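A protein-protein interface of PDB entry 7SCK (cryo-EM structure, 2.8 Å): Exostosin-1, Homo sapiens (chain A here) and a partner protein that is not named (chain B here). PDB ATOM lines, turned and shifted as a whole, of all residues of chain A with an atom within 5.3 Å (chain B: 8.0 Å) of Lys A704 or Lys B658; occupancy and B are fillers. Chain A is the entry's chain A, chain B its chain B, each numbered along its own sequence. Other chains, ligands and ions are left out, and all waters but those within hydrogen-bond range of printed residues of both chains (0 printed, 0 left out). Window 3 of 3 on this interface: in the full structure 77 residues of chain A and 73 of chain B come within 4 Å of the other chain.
Of chain B, only Lys B658 (2.9 Å) comes within 4 Å of Lys A704. Of chain A, only Gln A648 and Lys A704 come within 4 Å of Lys B658. Printed residues of chain A within 4 Å of Asp B659: Gln A648. Printed residues of chain B within 4 Å of Gln A648: Tyr B657, Lys B658 and Asp B659. Phe B668 touches none of the printed residues of chain A. The nearest printed residue of chain A that does not touch Lys B658 is Phe A703 (5.0 Å).
O of Phe A703 sits at hydrogen-bond distance from NH1 of Arg B651 (2.8 Å). The backbone carbonyl oxygen (O) of Lys B658 lies within hydrogen-bond range of the side-chain amide nitrogen (NE2) of Gln A648, at 3.3 Å. The side-chain carboxylate of Asp B659 sits close to the side-chain amide nitrogen of Gln A648, at 2.3 Å. The backbone carbonyl oxygen of Lys A704 lies within hydrogen-bond range of the side-chain amino group of Lys B658 (2.9 Å). NE2 of Gln A648 sits close to O of Tyr B657.
OE1 of Gln A648 is in hydrogen-bond range of NZ of Lys A704 (2.7 Å). NH2 of Arg B651 lies within salt-bridge range of OD2 of Asp B653 (2.6 Å). The side-chain carboxylate (OE2) of Glu A718 is in hydrogen-bond range of the backbone NH (N) of Lys A704, at 2.9 Å.
Of the 8 printed residues of chain A, 4 touch a printed residue of chain B. Among the printed residues, 6 pairs touch across the chains.
N of Leu A702 touches NH1 of Arg B651, 3.9 Å away.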
ATOM      1  N   GLN A 648     -16.527  10.636 -11.763  1.00  0.00           N
ATOM      2  CA  GLN A 648     -17.738  10.460 -10.979  1.00  0.00           C
ATOM      3  C   GLN A 648     -18.633   9.362 -11.542  1.00  0.00           C
ATOM      4  O   GLN A 648     -19.798   9.253 -11.144  1.00  0.00           O
ATOM      5  CB  GLN A 648     -18.497  11.787 -10.914  1.00  0.00           C
ATOM      6  CG  GLN A 648     -19.469  11.943  -9.762  1.00  0.00           C
ATOM      7  CD  GLN A 648     -20.246  13.241  -9.847  1.00  0.00           C
ATOM      8  OE1 GLN A 648     -20.204  13.937 -10.863  1.00  0.00           O
ATOM      9  NE2 GLN A 648     -20.955  13.579  -8.780  1.00  0.00           N
ATOM     10  N   LEU A 702     -10.479  21.483 -12.793  1.00  0.00           N
ATOM     11  CA  LEU A 702     -11.570  22.270 -13.373  1.00  0.00           C
ATOM     12  C   LEU A 702     -12.745  21.380 -13.775  1.00  0.00           C
ATOM     13  O   LEU A 702     -13.322  21.539 -14.852  1.00  0.00           O
ATOM     14  CB  LEU A 702     -11.090  23.105 -14.567  1.00  0.00           C
ATOM     15  CG  LEU A 702      -9.813  23.921 -14.361  1.00  0.00           C
ATOM     16  CD1 LEU A 702      -9.312  24.464 -15.679  1.00  0.00           C
ATOM     17  CD2 LEU A 702     -10.056  25.046 -13.374  1.00  0.00           C
ATOM     18  N   PHE A 703     -13.104  20.438 -12.908  1.00  0.00           N
ATOM     19  CA  PHE A 703     -14.260  19.577 -13.125  1.00  0.00           C
ATOM     20  C   PHE A 703     -15.456  20.164 -12.391  1.00  0.00           C
ATOM     21  O   PHE A 703     -15.388  20.401 -11.181  1.00  0.00           O
ATOM     22  CB  PHE A 703     -13.984  18.153 -12.647  1.00  0.00           C
ATOM     23  CG  PHE A 703     -15.207  17.274 -12.620  1.00  0.00           C
ATOM     24  CD1 PHE A 703     -15.688  16.700 -13.783  1.00  0.00           C
ATOM     25  CD2 PHE A 703     -15.869  17.020 -11.431  1.00  0.00           C
ATOM     26  CE1 PHE A 703     -16.810  15.891 -13.761  1.00  0.00           C
ATOM     27  CE2 PHE A 703     -16.989  16.212 -11.402  1.00  0.00           C
ATOM     28  CZ  PHE A 703     -17.461  15.649 -12.566  1.00  0.00           C
ATOM     29  N   LYS A 704     -16.546  20.395 -13.123  1.00  0.00           N
ATOM     30  CA  LYS A 704     -17.735  21.054 -12.581  1.00  0.00           C
ATOM     31  C   LYS A 704     -17.378  22.394 -11.944  1.00  0.00           C
ATOM     32  O   LYS A 704     -18.021  22.839 -10.991  1.00  0.00           O
ATOM     33  CB  LYS A 704     -18.469  20.154 -11.585  1.00  0.00           C
ATOM     34  CG  LYS A 704     -19.159  18.964 -12.228  1.00  0.00           C
ATOM     35  CD  LYS A 704     -19.976  18.180 -11.216  1.00  0.00           C
ATOM     36  CE  LYS A 704     -20.724  17.036 -11.881  1.00  0.00           C
ATOM     37  NZ  LYS A 704     -21.521  16.251 -10.899  1.00  0.00           N
ATOM     38  N   ASP A 705     -16.344  23.039 -12.475  1.00  0.00           N
ATOM     39  CA  ASP A 705     -15.882  24.329 -11.991  1.00  0.00           C
ATOM     40  C   ASP A 705     -16.392  25.424 -12.916  1.00  0.00           C
ATOM     41  O   ASP A 705     -16.449  25.245 -14.136  1.00  0.00           O
ATOM     42  CB  ASP A 705     -14.353  24.366 -11.913  1.00  0.00           C
ATOM     43  CG  ASP A 705     -13.836  25.594 -11.191  1.00  0.00           C
ATOM     44  OD1 ASP A 705     -14.655  26.340 -10.616  1.00  0.00           O
ATOM     45  OD2 ASP A 705     -12.606  25.814 -11.199  1.00  0.00           O
ATOM     46  N   GLN A 706     -16.765  26.561 -12.329  1.00  0.00           N
ATOM     47  CA  GLN A 706     -17.380  27.655 -13.079  1.00  0.00           C
ATOM     48  C   GLN A 706     -16.307  28.359 -13.904  1.00  0.00           C
ATOM     49  O   GLN A 706     -15.813  29.437 -13.567  1.00  0.00           O
ATOM     50  CB  GLN A 706     -18.089  28.619 -12.137  1.00  0.00           C
ATOM     51  CG  GLN A 706     -19.305  28.023 -11.446  1.00  0.00           C
ATOM     52  CD  GLN A 706     -20.034  29.032 -10.580  1.00  0.00           C
ATOM     53  OE1 GLN A 706     -19.637  30.193 -10.491  1.00  0.00           O
ATOM     54  NE2 GLN A 706     -21.110  28.591  -9.936  1.00  0.00           N
ATOM     55  N   LYS A 712     -11.517  24.173 -20.586  1.00  0.00           N
ATOM     56  CA  LYS A 712     -11.353  22.823 -20.076  1.00  0.00           C
ATOM     57  C   LYS A 712     -10.804  21.906 -21.163  1.00  0.00           C
ATOM     58  O   LYS A 712     -11.008  22.124 -22.360  1.00  0.00           O
ATOM     59  CB  LYS A 712     -12.684  22.272 -19.565  1.00  0.00           C
ATOM     60  CG  LYS A 712     -13.330  23.094 -18.468  1.00  0.00           C
ATOM     61  CD  LYS A 712     -14.613  22.447 -17.992  1.00  0.00           C
ATOM     62  CE  LYS A 712     -15.297  23.293 -16.941  1.00  0.00           C
ATOM     63  NZ  LYS A 712     -16.565  22.671 -16.479  1.00  0.00           N
ATOM     64  N   GLU A 718     -18.348  15.484 -18.235  1.00  0.00           N
ATOM     65  CA  GLU A 718     -19.611  15.899 -17.633  1.00  0.00           C
ATOM     66  C   GLU A 718     -20.796  15.453 -18.479  1.00  0.00           C
ATOM     67  O   GLU A 718     -21.827  15.029 -17.944  1.00  0.00           O
ATOM     68  CB  GLU A 718     -19.628  17.414 -17.442  1.00  0.00           C
ATOM     69  CG  GLU A 718     -18.492  17.947 -16.586  1.00  0.00           C
ATOM     70  CD  GLU A 718     -18.521  19.458 -16.455  1.00  0.00           C
ATOM     71  OE1 GLU A 718     -19.440  20.088 -17.019  1.00  0.00           O
ATOM     72  OE2 GLU A 718     -17.623  20.016 -15.788  1.00  0.00           O
ATOM     73  N   PRO B 604     -11.571  21.670  -5.581  1.00  0.00           N
ATOM     74  CA  PRO B 604     -11.586  22.610  -6.707  1.00  0.00           C
ATOM     75  C   PRO B 604     -11.356  24.058  -6.312  1.00  0.00           C
ATOM     76  O   PRO B 604     -11.348  24.926  -7.193  1.00  0.00           O
ATOM     77  CB  PRO B 604     -12.999  22.424  -7.274  1.00  0.00           C
ATOM     78  CG  PRO B 604     -13.813  22.077  -6.083  1.00  0.00           C
ATOM     79  CD  PRO B 604     -12.929  21.232  -5.214  1.00  0.00           C
ATOM     80  N   ARG B 651      -6.979  16.321  -9.221  1.00  0.00           N
ATOM     81  CA  ARG B 651      -7.715  17.125  -8.260  1.00  0.00           C
ATOM     82  C   ARG B 651      -8.485  16.134  -7.398  1.00  0.00           C
ATOM     83  O   ARG B 651      -9.635  15.803  -7.687  1.00  0.00           O
ATOM     84  CB  ARG B 651      -8.643  18.100  -8.946  1.00  0.00           C
ATOM     85  CG  ARG B 651      -9.322  19.059  -8.008  1.00  0.00           C
ATOM     86  CD  ARG B 651     -10.471  19.763  -8.690  1.00  0.00           C
ATOM     87  NE  ARG B 651     -11.665  18.931  -8.738  1.00  0.00           N
ATOM     88  CZ  ARG B 651     -12.805  19.294  -9.309  1.00  0.00           C
ATOM     89  NH1 ARG B 651     -12.935  20.467  -9.905  1.00  0.00           N
ATOM     90  NH2 ARG B 651     -13.840  18.460  -9.282  1.00  0.00           N
ATOM     91  N   ASP B 653     -10.832  14.628  -4.991  1.00  0.00           N
ATOM     92  CA  ASP B 653     -12.108  15.086  -4.479  1.00  0.00           C
ATOM     93  C   ASP B 653     -12.705  14.024  -3.574  1.00  0.00           C
ATOM     94  O   ASP B 653     -12.344  12.846  -3.664  1.00  0.00           O
ATOM     95  CB  ASP B 653     -13.085  15.396  -5.622  1.00  0.00           C
ATOM     96  CG  ASP B 653     -12.807  16.728  -6.282  1.00  0.00           C
ATOM     97  OD1 ASP B 653     -11.733  17.307  -6.023  1.00  0.00           O
ATOM     98  OD2 ASP B 653     -13.668  17.205  -7.050  1.00  0.00           O
ATOM     99  N   PRO B 654     -13.601  14.405  -2.669  1.00  0.00           N
ATOM    100  CA  PRO B 654     -14.360  13.391  -1.939  1.00  0.00           C
ATOM    101  C   PRO B 654     -15.160  12.541  -2.909  1.00  0.00           C
ATOM    102  O   PRO B 654     -15.672  13.033  -3.914  1.00  0.00           O
ATOM    103  CB  PRO B 654     -15.277  14.215  -1.031  1.00  0.00           C
ATOM    104  CG  PRO B 654     -14.641  15.545  -0.944  1.00  0.00           C
ATOM    105  CD  PRO B 654     -13.968  15.768  -2.258  1.00  0.00           C
ATOM    106  N   VAL B 655     -15.254  11.248  -2.611  1.00  0.00           N
ATOM    107  CA  VAL B 655     -16.174  10.417  -3.361  1.00  0.00           C
ATOM    108  C   VAL B 655     -17.602  10.847  -3.046  1.00  0.00           C
ATOM    109  O   VAL B 655     -17.880  11.485  -2.025  1.00  0.00           O
ATOM    110  CB  VAL B 655     -15.949   8.929  -3.053  1.00  0.00           C
ATOM    111  CG1 VAL B 655     -14.472   8.599  -3.113  1.00  0.00           C
ATOM    112  CG2 VAL B 655     -16.518   8.578  -1.691  1.00  0.00           C
ATOM    113  N   LEU B 656     -18.520  10.502  -3.947  1.00  0.00           N
ATOM    114  CA  LEU B 656     -19.897  11.000  -3.899  1.00  0.00           C
ATOM    115  C   LEU B 656     -19.944  12.525  -3.971  1.00  0.00           C
ATOM    116  O   LEU B 656     -20.779  13.163  -3.325  1.00  0.00           O
ATOM    117  CB  LEU B 656     -20.638  10.510  -2.649  1.00  0.00           C
ATOM    118  CG  LEU B 656     -20.716   9.012  -2.377  1.00  0.00           C
ATOM    119  CD1 LEU B 656     -21.727   8.742  -1.278  1.00  0.00           C
ATOM    120  CD2 LEU B 656     -21.075   8.253  -3.644  1.00  0.00           C
ATOM    121  N   TYR B 657     -19.050  13.120  -4.758  1.00  0.00           N
ATOM    122  CA  TYR B 657     -18.961  14.570  -4.852  1.00  0.00           C
ATOM    123  C   TYR B 657     -20.020  15.100  -5.807  1.00  0.00           C
ATOM    124  O   TYR B 657     -20.134  14.631  -6.942  1.00  0.00           O
ATOM    125  CB  TYR B 657     -17.568  14.984  -5.319  1.00  0.00           C
ATOM    126  CG  TYR B 657     -17.303  16.468  -5.243  1.00  0.00           C
ATOM    127  CD1 TYR B 657     -17.304  17.129  -4.025  1.00  0.00           C
ATOM    128  CD2 TYR B 657     -17.038  17.205  -6.389  1.00  0.00           C
ATOM    129  CE1 TYR B 657     -17.060  18.487  -3.952  1.00  0.00           C
ATOM    130  CE2 TYR B 657     -16.792  18.562  -6.326  1.00  0.00           C
ATOM    131  CZ  TYR B 657     -16.804  19.196  -5.105  1.00  0.00           C
ATOM    132  OH  TYR B 657     -16.560  20.548  -5.034  1.00  0.00           O
ATOM    133  N   LYS B 658     -20.791  16.083  -5.342  1.00  0.00           N
ATOM    134  CA  LYS B 658     -21.851  16.711  -6.131  1.00  0.00           C
ATOM    135  C   LYS B 658     -22.837  15.688  -6.686  1.00  0.00           C
ATOM    136  O   LYS B 658     -23.229  15.758  -7.853  1.00  0.00           O
ATOM    137  CB  LYS B 658     -21.272  17.565  -7.262  1.00  0.00           C
ATOM    138  CG  LYS B 658     -20.579  18.831  -6.783  1.00  0.00           C
ATOM    139  CD  LYS B 658     -20.252  19.758  -7.941  1.00  0.00           C
ATOM    140  CE  LYS B 658     -19.646  21.062  -7.450  1.00  0.00           C
ATOM    141  NZ  LYS B 658     -19.355  22.001  -8.568  1.00  0.00           N
ATOM    142  N   ASP B 659     -23.240  14.729  -5.861  1.00  0.00           N
ATOM    143  CA  ASP B 659     -24.219  13.735  -6.265  1.00  0.00           C
ATOM    144  C   ASP B 659     -25.575  14.017  -5.625  1.00  0.00           C
ATOM    145  O   ASP B 659     -25.710  14.839  -4.715  1.00  0.00           O
ATOM    146  CB  ASP B 659     -23.738  12.335  -5.902  1.00  0.00           C
ATOM    147  CG  ASP B 659     -22.669  11.835  -6.841  1.00  0.00           C
ATOM    148  OD1 ASP B 659     -22.671  12.257  -8.015  1.00  0.00           O
ATOM    149  OD2 ASP B 659     -21.829  11.018  -6.415  1.00  0.00           O
ATOM    150  N   ASP B 660     -26.595  13.319  -6.121  1.00  0.00           N
ATOM    151  CA  ASP B 660     -27.953  13.454  -5.593  1.00  0.00           C
ATOM    152  C   ASP B 660     -28.125  12.551  -4.372  1.00  0.00           C
ATOM    153  O   ASP B 660     -28.958  11.646  -4.327  1.00  0.00           O
ATOM    154  CB  ASP B 660     -28.978  13.137  -6.676  1.00  0.00           C
ATOM    155  CG  ASP B 660     -30.376  13.598  -6.308  1.00  0.00           C
ATOM    156  OD1 ASP B 660     -30.535  14.227  -5.241  1.00  0.00           O
ATOM    157  OD2 ASP B 660     -31.316  13.333  -7.087  1.00  0.00           O
ATOM    158  N   PHE B 661     -27.305  12.826  -3.365  1.00  0.00           N
ATOM    159  CA  PHE B 661     -27.235  12.053  -2.141  1.00  0.00           C
ATOM    160  C   PHE B 661     -27.571  12.937  -0.948  1.00  0.00           C
ATOM    161  O   PHE B 661     -27.351  14.153  -0.994  1.00  0.00           O
ATOM    162  CB  PHE B 661     -25.832  11.458  -1.964  1.00  0.00           C
ATOM    163  CG  PHE B 661     -25.813  10.155  -1.228  1.00  0.00           C
ATOM    164  CD1 PHE B 661     -26.380   9.020  -1.786  1.00  0.00           C
ATOM    165  CD2 PHE B 661     -25.215  10.056   0.015  1.00  0.00           C
ATOM    166  CE1 PHE B 661     -26.361   7.815  -1.112  1.00  0.00           C
ATOM    167  CE2 PHE B 661     -25.191   8.854   0.693  1.00  0.00           C
ATOM    168  CZ  PHE B 661     -25.765   7.731   0.130  1.00  0.00           C
ATOM    169  N   GLU B 663     -27.205  14.986   2.396  1.00  0.00           N
ATOM    170  CA  GLU B 663     -26.027  15.695   2.885  1.00  0.00           C
ATOM    171  C   GLU B 663     -25.484  15.083   4.170  1.00  0.00           C
ATOM    172  O   GLU B 663     -24.268  15.103   4.395  1.00  0.00           O
ATOM    173  CB  GLU B 663     -26.362  17.170   3.108  1.00  0.00           C
ATOM    174  CG  GLU B 663     -27.005  17.854   1.908  1.00  0.00           C
ATOM    175  CD  GLU B 663     -26.050  18.014   0.741  1.00  0.00           C
ATOM    176  OE1 GLU B 663     -24.822  17.996   0.965  1.00  0.00           O
ATOM    177  OE2 GLU B 663     -26.530  18.160  -0.403  1.00  0.00           O
ATOM    178  N   LYS B 666     -22.993  12.159   3.659  1.00  0.00           N
ATOM    179  CA  LYS B 666     -21.730  12.492   3.017  1.00  0.00           C
ATOM    180  C   LYS B 666     -20.636  12.694   4.057  1.00  0.00           C
ATOM    181  O   LYS B 666     -20.877  13.208   5.152  1.00  0.00           O
ATOM    182  CB  LYS B 666     -21.875  13.755   2.171  1.00  0.00           C
ATOM    183  CG  LYS B 666     -22.671  13.574   0.892  1.00  0.00           C
ATOM    184  CD  LYS B 666     -22.549  14.807   0.013  1.00  0.00           C
ATOM    185  CE  LYS B 666     -23.181  14.592  -1.348  1.00  0.00           C
ATOM    186  NZ  LYS B 666     -22.970  15.769  -2.233  1.00  0.00           N
ATOM    187  N   PHE B 668     -17.864  14.648   3.649  1.00  0.00           N
ATOM    188  CA  PHE B 668     -17.464  16.053   3.632  1.00  0.00           C
ATOM    189  C   PHE B 668     -18.460  16.858   2.809  1.00  0.00           C
ATOM    190  O   PHE B 668     -18.151  17.297   1.695  1.00  0.00           O
ATOM    191  CB  PHE B 668     -16.051  16.204   3.072  1.00  0.00           C
ATOM    192  CG  PHE B 668     -15.039  15.315   3.734  1.00  0.00           C
ATOM    193  CD1 PHE B 668     -14.688  15.511   5.054  1.00  0.00           C
ATOM    194  CD2 PHE B 668     -14.426  14.300   3.033  1.00  0.00           C
ATOM    195  CE1 PHE B 668     -13.756  14.703   5.661  1.00  0.00           C
ATOM    196  CE2 PHE B 668     -13.496  13.491   3.632  1.00  0.00           C
ATOM    197  CZ  PHE B 668     -13.160  13.690   4.947  1.00  0.00           C
ATOM    198  N   ILE B 671     -17.785  21.142   0.734  1.00  0.00           N
ATOM    199  CA  ILE B 671     -16.751  21.513  -0.225  1.00  0.00           C
ATOM    200  C   ILE B 671     -17.432  22.104  -1.451  1.00  0.00           C
ATOM    201  O   ILE B 671     -18.255  21.438  -2.093  1.00  0.00           O
ATOM    202  CB  ILE B 671     -15.860  20.322  -0.615  1.00  0.00           C
ATOM    203  CG1 ILE B 671     -15.041  19.848   0.583  1.00  0.00           C
ATOM    204  CG2 ILE B 671     -14.936  20.705  -1.756  1.00  0.00           C
ATOM    205  CD1 ILE B 671     -13.766  19.120   0.204  1.00  0.00           C
ATOM    206  N   GLY B 672     -17.089  23.348  -1.775  1.00  0.00           N
ATOM    207  CA  GLY B 672     -17.638  24.014  -2.938  1.00  0.00           C
ATOM    208  C   GLY B 672     -17.045  25.391  -3.152  1.00  0.00           C
ATOM    209  O   GLY B 672     -16.977  26.197  -2.222  1.00  0.00           O
ATOM    210  N   SER B 673     -16.616  25.671  -4.378  1.00  0.00           N
ATOM    211  CA  SER B 673     -16.010  26.956  -4.700  1.00  0.00           C
ATOM    212  C   SER B 673     -16.106  27.250  -6.194  1.00  0.00           C
ATOM    213  O   SER B 673     -15.116  27.615  -6.830  1.00  0.00           O
ATOM    214  CB  SER B 673     -14.550  26.986  -4.249  1.00  0.00           C
ATOM    215  OG  SER B 673     -13.946  28.227  -4.563  1.00  0.00           O
